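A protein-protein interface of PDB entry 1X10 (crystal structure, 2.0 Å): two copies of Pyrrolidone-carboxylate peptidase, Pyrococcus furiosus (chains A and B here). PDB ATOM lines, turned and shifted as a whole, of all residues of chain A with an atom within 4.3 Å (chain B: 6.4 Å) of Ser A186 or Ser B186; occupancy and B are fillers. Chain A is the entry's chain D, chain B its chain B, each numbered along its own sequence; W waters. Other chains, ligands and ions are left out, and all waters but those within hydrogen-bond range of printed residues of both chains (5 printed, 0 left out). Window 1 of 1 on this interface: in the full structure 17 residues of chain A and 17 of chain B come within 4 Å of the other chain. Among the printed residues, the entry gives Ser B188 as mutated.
O of Ser B186 sits close to O of Ser A186 (3.2 Å).
The side-chain hydroxyl of Ser B188 lies within hydrogen-bond range of the backbone NH of Met B191.
Of the 15 printed residues of chain B, 5 touch a printed residue of chain A. Printed residues of chain B that touch a printed residue of chain A: Ser B74, Pro B130, Pro B185, Ser B186 and Met B191. Hydrophobic or aromatic side chains of chain A within 4 Å of the printed part of chain B: Pro A171, Ile A174 and Pro A185. Along chain A the printed residues that touch a printed residue of chain B span positions 171 to 186. Among the printed residues, 7 pairs touch across the chains. Among the printed residues, no Asp or Glu carboxylate lies within 4 Å of a Lys or Arg side-chain nitrogen of the other chain.
Pro B185 touches its own counterpart, Pro A185. Ser B186 touches its own counterpart, Ser A186. Positions printed for both chains: 169, 170, 171, 174, 184, 185, 186 and 187. Of the 7 pairs that touch across the chains among the printed residues, 2 have their exchanged pair printed and touching as well.
CB of Pro A171 touches CD of Pro B130, at 3.9 Å. Pro A171 touches Met B191. Ile A174 touches Pro B130. Pro A184 touches Ser B74 (O to OG, 3.8 Å). CA of Pro A185 touches CB of Ser B74, 3.9 Å away. CG of Pro A185 touches CG of Pro B185, at 3.9 Å.
Of chain B, only Ser B186 comes within 4 Å of Ser A186. Of chain A, only Ser A186 comes within 4 Å of Ser B186. Printed residues of chain A within 4 Å of Met B191: Pro A171 (3.8 Å). Printed residues of chain B within 4 Å of Pro A171: Pro B130 and Met B191. Of the printed residues of chain A, Ser B74 touches Pro A184 (3.8 Å) and Pro A185 (3.9 Å). The nearest residue of chain B that does not touch Ser A186 is Pro B130 (4.4 Å). The nearest printed residue of chain A that does not touch Pro B185 is Ser A186 (5.5 Å).
Water W3 lies within hydrogen-bond range of OG of Ser B186 (2.6 Å) and O of Ser A186 (2.9 Å). Water W4 bridges OG of Ser A186 and O of Ser B186. Water W1 lies within hydrogen-bond range of the side-chain hydroxyl of Ser A186 (2.7 Å), the backbone carbonyl oxygen of Ser B74 (2.8 Å) and the backbone carbonyl oxygen of Pro A184 (2.9 Å). Water W5 bridges the backbone carbonyl oxygen (O) of Ser A186 (2.8 Å) and the backbone NH (N) of Ser B186 (3.0 Å). Water W2 lies within hydrogen-bond range of the backbone carbonyl oxygen (O) of Ser B74, the backbone carbonyl oxygen (O) of Ser B186 and the backbone NH (N) of Ser A186.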
ATOM      1  N   TYR A 169      11.397  -1.811  12.288  1.00  0.00           N
ATOM      2  CA  TYR A 169      12.482  -1.034  11.702  1.00  0.00           C
ATOM      3  C   TYR A 169      11.792  -0.131  10.688  1.00  0.00           C
ATOM      4  O   TYR A 169      10.740  -0.502  10.165  1.00  0.00           O
ATOM      5  CB  TYR A 169      13.397  -1.923  10.855  1.00  0.00           C
ATOM      6  CG  TYR A 169      14.444  -2.744  11.563  1.00  0.00           C
ATOM      7  CD1 TYR A 169      15.455  -2.135  12.306  1.00  0.00           C
ATOM      8  CD2 TYR A 169      14.487  -4.129  11.397  1.00  0.00           C
ATOM      9  CE1 TYR A 169      16.495  -2.889  12.858  1.00  0.00           C
ATOM     10  CE2 TYR A 169      15.516  -4.887  11.938  1.00  0.00           C
ATOM     11  CZ  TYR A 169      16.519  -4.260  12.664  1.00  0.00           C
ATOM     12  OH  TYR A 169      17.558  -5.007  13.171  1.00  0.00           O
ATOM     13  N   ILE A 170      12.364   1.038  10.399  1.00  0.00           N
ATOM     14  CA  ILE A 170      11.794   1.851   9.337  1.00  0.00           C
ATOM     15  C   ILE A 170      12.627   1.398   8.123  1.00  0.00           C
ATOM     16  O   ILE A 170      13.751   0.912   8.281  1.00  0.00           O
ATOM     17  CB  ILE A 170      11.923   3.381   9.582  1.00  0.00           C
ATOM     18  CG1 ILE A 170      13.371   3.777   9.850  1.00  0.00           C
ATOM     19  CG2 ILE A 170      11.011   3.792  10.733  1.00  0.00           C
ATOM     20  CD1 ILE A 170      13.555   5.292   9.971  1.00  0.00           C
ATOM     21  N   PRO A 171      12.086   1.533   6.903  1.00  0.00           N
ATOM     22  CA  PRO A 171      12.768   1.119   5.671  1.00  0.00           C
ATOM     23  C   PRO A 171      14.265   1.400   5.514  1.00  0.00           C
ATOM     24  O   PRO A 171      15.022   0.509   5.136  1.00  0.00           O
ATOM     25  CB  PRO A 171      11.932   1.782   4.582  1.00  0.00           C
ATOM     26  CG  PRO A 171      10.552   1.706   5.165  1.00  0.00           C
ATOM     27  CD  PRO A 171      10.789   2.156   6.591  1.00  0.00           C
ATOM     28  N   ILE A 174      16.786  -1.074   6.807  1.00  0.00           N
ATOM     29  CA  ILE A 174      16.891  -2.379   6.171  1.00  0.00           C
ATOM     30  C   ILE A 174      17.999  -2.456   5.116  1.00  0.00           C
ATOM     31  O   ILE A 174      18.566  -3.526   4.873  1.00  0.00           O
ATOM     32  CB  ILE A 174      15.554  -2.762   5.486  1.00  0.00           C
ATOM     33  CG1 ILE A 174      14.393  -2.639   6.482  1.00  0.00           C
ATOM     34  CG2 ILE A 174      15.635  -4.179   4.940  1.00  0.00           C
ATOM     35  CD1 ILE A 174      14.546  -3.498   7.723  1.00  0.00           C
ATOM     36  N   PRO A 184      14.601  -8.215   6.990  1.00  0.00           N
ATOM     37  CA  PRO A 184      13.554  -8.091   8.008  1.00  0.00           C
ATOM     38  C   PRO A 184      12.458  -7.116   7.570  1.00  0.00           C
ATOM     39  O   PRO A 184      12.672  -6.279   6.694  1.00  0.00           O
ATOM     40  CB  PRO A 184      14.322  -7.601   9.234  1.00  0.00           C
ATOM     41  CG  PRO A 184      15.451  -6.826   8.643  1.00  0.00           C
ATOM     42  CD  PRO A 184      15.885  -7.684   7.480  1.00  0.00           C
ATOM     43  N   PRO A 185      11.265  -7.232   8.171  1.00  0.00           N
ATOM     44  CA  PRO A 185      10.121  -6.368   7.860  1.00  0.00           C
ATOM     45  C   PRO A 185      10.405  -4.930   8.284  1.00  0.00           C
ATOM     46  O   PRO A 185      11.283  -4.681   9.119  1.00  0.00           O
ATOM     47  CB  PRO A 185       8.987  -6.968   8.695  1.00  0.00           C
ATOM     48  CG  PRO A 185       9.426  -8.380   8.952  1.00  0.00           C
ATOM     49  CD  PRO A 185      10.897  -8.239   9.182  1.00  0.00           C
ATOM     50  N   SER A 186       9.659  -3.989   7.713  1.00  0.00           N
ATOM     51  CA  SER A 186       9.812  -2.581   8.063  1.00  0.00           C
ATOM     52  C   SER A 186       8.467  -1.877   7.936  1.00  0.00           C
ATOM     53  O   SER A 186       7.533  -2.415   7.345  1.00  0.00           O
ATOM     54  CB  SER A 186      10.857  -1.906   7.167  1.00  0.00           C
ATOM     55  OG  SER A 186      10.526  -2.010   5.790  1.00  0.00           O
ATOM     56  N   MET A 187       8.375  -0.684   8.515  1.00  0.00           N
ATOM     57  CA  MET A 187       7.155   0.118   8.472  1.00  0.00           C
ATOM     58  C   MET A 187       7.605   1.572   8.404  1.00  0.00           C
ATOM     59  O   MET A 187       8.519   1.977   9.117  1.00  0.00           O
ATOM     60  CB  MET A 187       6.308  -0.129   9.724  1.00  0.00           C
ATOM     61  CG  MET A 187       5.006   0.659   9.753  1.00  0.00           C
ATOM     62  SD  MET A 187       3.947   0.174  11.129  1.00  0.00           S
ATOM     63  CE  MET A 187       3.115  -1.261  10.430  1.00  0.00           C
ATOM     64  N   ARG B  73       6.491 -11.302   1.299  1.00  0.00           N
ATOM     65  CA  ARG B  73       7.811 -10.711   1.119  1.00  0.00           C
ATOM     66  C   ARG B  73       7.872  -9.350   1.804  1.00  0.00           C
ATOM     67  O   ARG B  73       6.898  -8.602   1.802  1.00  0.00           O
ATOM     68  CB  ARG B  73       8.168 -10.663  -0.371  1.00  0.00           C
ATOM     69  CG  ARG B  73       8.816 -11.989  -0.766  1.00  0.00           C
ATOM     70  CD  ARG B  73       8.319 -12.613  -2.050  1.00  0.00           C
ATOM     71  NE  ARG B  73       9.061 -12.147  -3.209  1.00  0.00           N
ATOM     72  CZ  ARG B  73       9.442 -12.916  -4.226  1.00  0.00           C
ATOM     73  NH1 ARG B  73       9.168 -14.211  -4.246  1.00  0.00           N
ATOM     74  NH2 ARG B  73      10.087 -12.375  -5.246  1.00  0.00           N
ATOM     75  N   SER B  74       9.021  -9.063   2.410  1.00  0.00           N
ATOM     76  CA  SER B  74       9.242  -7.846   3.196  1.00  0.00           C
ATOM     77  C   SER B  74       9.857  -6.654   2.483  1.00  0.00           C
ATOM     78  O   SER B  74       9.933  -5.568   3.050  1.00  0.00           O
ATOM     79  CB  SER B  74      10.133  -8.186   4.391  1.00  0.00           C
ATOM     80  OG  SER B  74      11.402  -8.623   3.924  1.00  0.00           O
ATOM     81  N   PRO B 130      14.252  -0.654   0.519  1.00  0.00           N
ATOM     82  CA  PRO B 130      14.778  -2.019   0.622  1.00  0.00           C
ATOM     83  C   PRO B 130      14.376  -2.857  -0.590  1.00  0.00           C
ATOM     84  O   PRO B 130      13.210  -2.878  -0.996  1.00  0.00           O
ATOM     85  CB  PRO B 130      14.183  -2.536   1.938  1.00  0.00           C
ATOM     86  CG  PRO B 130      12.993  -1.659   2.176  1.00  0.00           C
ATOM     87  CD  PRO B 130      13.435  -0.305   1.691  1.00  0.00           C
ATOM     88  N   PRO B 168       5.587  -6.080  -1.844  1.00  0.00           N
ATOM     89  CA  PRO B 168       4.953  -6.671  -0.663  1.00  0.00           C
ATOM     90  C   PRO B 168       3.511  -6.192  -0.567  1.00  0.00           C
ATOM     91  O   PRO B 168       3.065  -5.370  -1.367  1.00  0.00           O
ATOM     92  CB  PRO B 168       5.785  -6.123   0.499  1.00  0.00           C
ATOM     93  CG  PRO B 168       7.120  -5.778  -0.138  1.00  0.00           C
ATOM     94  CD  PRO B 168       6.714  -5.209  -1.468  1.00  0.00           C
ATOM     95  N   TYR B 169       2.785  -6.716   0.413  1.00  0.00           N
ATOM     96  CA  TYR B 169       1.415  -6.275   0.666  1.00  0.00           C
ATOM     97  C   TYR B 169       1.564  -4.817   1.071  1.00  0.00           C
ATOM     98  O   TYR B 169       2.609  -4.446   1.608  1.00  0.00           O
ATOM     99  CB  TYR B 169       0.847  -6.954   1.912  1.00  0.00           C
ATOM    100  CG  TYR B 169       0.312  -8.351   1.778  1.00  0.00           C
ATOM    101  CD1 TYR B 169      -0.774  -8.628   0.947  1.00  0.00           C
ATOM    102  CD2 TYR B 169       0.809  -9.376   2.585  1.00  0.00           C
ATOM    103  CE1 TYR B 169      -1.364  -9.893   0.932  1.00  0.00           C
ATOM    104  CE2 TYR B 169       0.227 -10.639   2.581  1.00  0.00           C
ATOM    105  CZ  TYR B 169      -0.856 -10.888   1.758  1.00  0.00           C
ATOM    106  OH  TYR B 169      -1.447 -12.125   1.779  1.00  0.00           O
ATOM    107  N   ILE B 170       0.546  -3.990   0.830  1.00  0.00           N
ATOM    108  CA  ILE B 170       0.622  -2.623   1.325  1.00  0.00           C
ATOM    109  C   ILE B 170      -0.083  -2.742   2.683  1.00  0.00           C
ATOM    110  O   ILE B 170      -0.906  -3.645   2.888  1.00  0.00           O
ATOM    111  CB  ILE B 170      -0.078  -1.580   0.405  1.00  0.00           C
ATOM    112  CG1 ILE B 170      -1.523  -1.979   0.120  1.00  0.00           C
ATOM    113  CG2 ILE B 170       0.722  -1.421  -0.888  1.00  0.00           C
ATOM    114  CD1 ILE B 170      -2.270  -0.924  -0.682  1.00  0.00           C
ATOM    115  N   PRO B 171       0.235  -1.854   3.635  1.00  0.00           N
ATOM    116  CA  PRO B 171      -0.358  -1.879   4.978  1.00  0.00           C
ATOM    117  C   PRO B 171      -1.848  -2.188   5.136  1.00  0.00           C
ATOM    118  O   PRO B 171      -2.216  -3.037   5.947  1.00  0.00           O
ATOM    119  CB  PRO B 171       0.022  -0.511   5.540  1.00  0.00           C
ATOM    120  CG  PRO B 171       1.375  -0.288   4.930  1.00  0.00           C
ATOM    121  CD  PRO B 171       1.129  -0.693   3.484  1.00  0.00           C
ATOM    122  N   GLU B 172      -2.707  -1.515   4.377  1.00  0.00           N
ATOM    123  CA  GLU B 172      -4.143  -1.753   4.505  1.00  0.00           C
ATOM    124  C   GLU B 172      -4.552  -3.205   4.270  1.00  0.00           C
ATOM    125  O   GLU B 172      -5.594  -3.647   4.757  1.00  0.00           O
ATOM    126  CB  GLU B 172      -4.925  -0.836   3.560  1.00  0.00           C
ATOM    127  CG  GLU B 172      -4.531  -0.947   2.104  1.00  0.00           C
ATOM    128  CD  GLU B 172      -5.180   0.126   1.262  1.00  0.00           C
ATOM    129  OE1 GLU B 172      -6.320  -0.085   0.804  1.00  0.00           O
ATOM    130  OE2 GLU B 172      -4.549   1.189   1.076  1.00  0.00           O
ATOM    131  N   ILE B 174      -3.014  -5.750   5.412  1.00  0.00           N
ATOM    132  CA  ILE B 174      -2.656  -6.524   6.596  1.00  0.00           C
ATOM    133  C   ILE B 174      -3.744  -6.534   7.672  1.00  0.00           C
ATOM    134  O   ILE B 174      -3.858  -7.494   8.436  1.00  0.00           O
ATOM    135  CB  ILE B 174      -1.355  -5.968   7.241  1.00  0.00           C
ATOM    136  CG1 ILE B 174      -0.248  -5.866   6.190  1.00  0.00           C
ATOM    137  CG2 ILE B 174      -0.924  -6.854   8.397  1.00  0.00           C
ATOM    138  CD1 ILE B 174       0.109  -7.182   5.538  1.00  0.00           C
ATOM    139  N   PRO B 184       1.860 -10.571   8.397  1.00  0.00           N
ATOM    140  CA  PRO B 184       2.873 -10.525   7.342  1.00  0.00           C
ATOM    141  C   PRO B 184       3.437  -9.111   7.157  1.00  0.00           C
ATOM    142  O   PRO B 184       2.815  -8.124   7.558  1.00  0.00           O
ATOM    143  CB  PRO B 184       2.111 -11.022   6.112  1.00  0.00           C
ATOM    144  CG  PRO B 184       0.711 -10.582   6.381  1.00  0.00           C
ATOM    145  CD  PRO B 184       0.532 -10.890   7.847  1.00  0.00           C
ATOM    146  N   PRO B 185       4.633  -9.006   6.558  1.00  0.00           N
ATOM    147  CA  PRO B 185       5.298  -7.721   6.307  1.00  0.00           C
ATOM    148  C   PRO B 185       4.508  -6.908   5.290  1.00  0.00           C
ATOM    149  O   PRO B 185       3.702  -7.461   4.543  1.00  0.00           O
ATOM    150  CB  PRO B 185       6.659  -8.133   5.740  1.00  0.00           C
ATOM    151  CG  PRO B 185       6.853  -9.535   6.228  1.00  0.00           C
ATOM    152  CD  PRO B 185       5.476 -10.123   6.106  1.00  0.00           C
ATOM    153  N   SER B 186       4.746  -5.602   5.261  1.00  0.00           N
ATOM    154  CA  SER B 186       4.076  -4.721   4.319  1.00  0.00           C
ATOM    155  C   SER B 186       5.011  -3.569   3.966  1.00  0.00           C
ATOM    156  O   SER B 186       6.021  -3.359   4.637  1.00  0.00           O
ATOM    157  CB  SER B 186       2.763  -4.184   4.907  1.00  0.00           C
ATOM    158  OG  SER B 186       2.965  -3.469   6.114  1.00  0.00           O
ATOM    159  N   MET B 187       4.677  -2.847   2.902  1.00  0.00           N
ATOM    160  CA  MET B 187       5.466  -1.707   2.440  1.00  0.00           C
ATOM    161  C   MET B 187       4.458  -0.718   1.860  1.00  0.00           C
ATOM    162  O   MET B 187       3.536  -1.118   1.148  1.00  0.00           O
ATOM    163  CB  MET B 187       6.466  -2.151   1.367  1.00  0.00           C
ATOM    164  CG  MET B 187       7.344  -1.025   0.833  1.00  0.00           C
ATOM    165  SD  MET B 187       8.648  -1.631  -0.253  1.00  0.00           S
ATOM    166  CE  MET B 187       9.906  -2.086   0.933  1.00  0.00           C
ATOM    167  N   SER B 188       4.623   0.562   2.177  1.00  0.00           N
ATOM    168  CA  SER B 188       3.694   1.586   1.709  1.00  0.00           C
ATOM    169  C   SER B 188       3.485   1.560   0.203  1.00  0.00           C
ATOM    170  O   SER B 188       4.390   1.202  -0.559  1.00  0.00           O
ATOM    171  CB  SER B 188       4.180   2.984   2.111  1.00  0.00           C
ATOM    172  OG  SER B 188       5.253   3.400   1.281  1.00  0.00           O
ATOM    173  N   MET B 191       5.942   3.841  -1.628  1.00  0.00           N
ATOM    174  CA  MET B 191       7.287   3.325  -1.859  1.00  0.00           C
ATOM    175  C   MET B 191       7.301   2.298  -2.984  1.00  0.00           C
ATOM    176  O   MET B 191       8.249   2.252  -3.776  1.00  0.00           O
ATOM    177  CB  MET B 191       7.858   2.693  -0.587  1.00  0.00           C
ATOM    178  CG  MET B 191       9.259   2.139  -0.773  1.00  0.00           C
ATOM    179  SD  MET B 191      10.043   1.684   0.791  1.00  0.00           S
ATOM    180  CE  MET B 191      10.625   3.320   1.338  1.00  0.00           C
HETATM  181  O   HOH W   1      11.681  -4.313   4.880  1.00  0.00           O
HETATM  182  O   HOH W   2       8.247  -5.091   5.322  1.00  0.00           O
HETATM  183  O   HOH W   3       4.720  -1.692   6.940  1.00  0.00           O
HETATM  184  O   HOH W   4       8.299  -1.534   4.377  1.00  0.00           O
HETATM  185  O   HOH W   5       6.200  -4.856   7.725  1.00  0.00           O
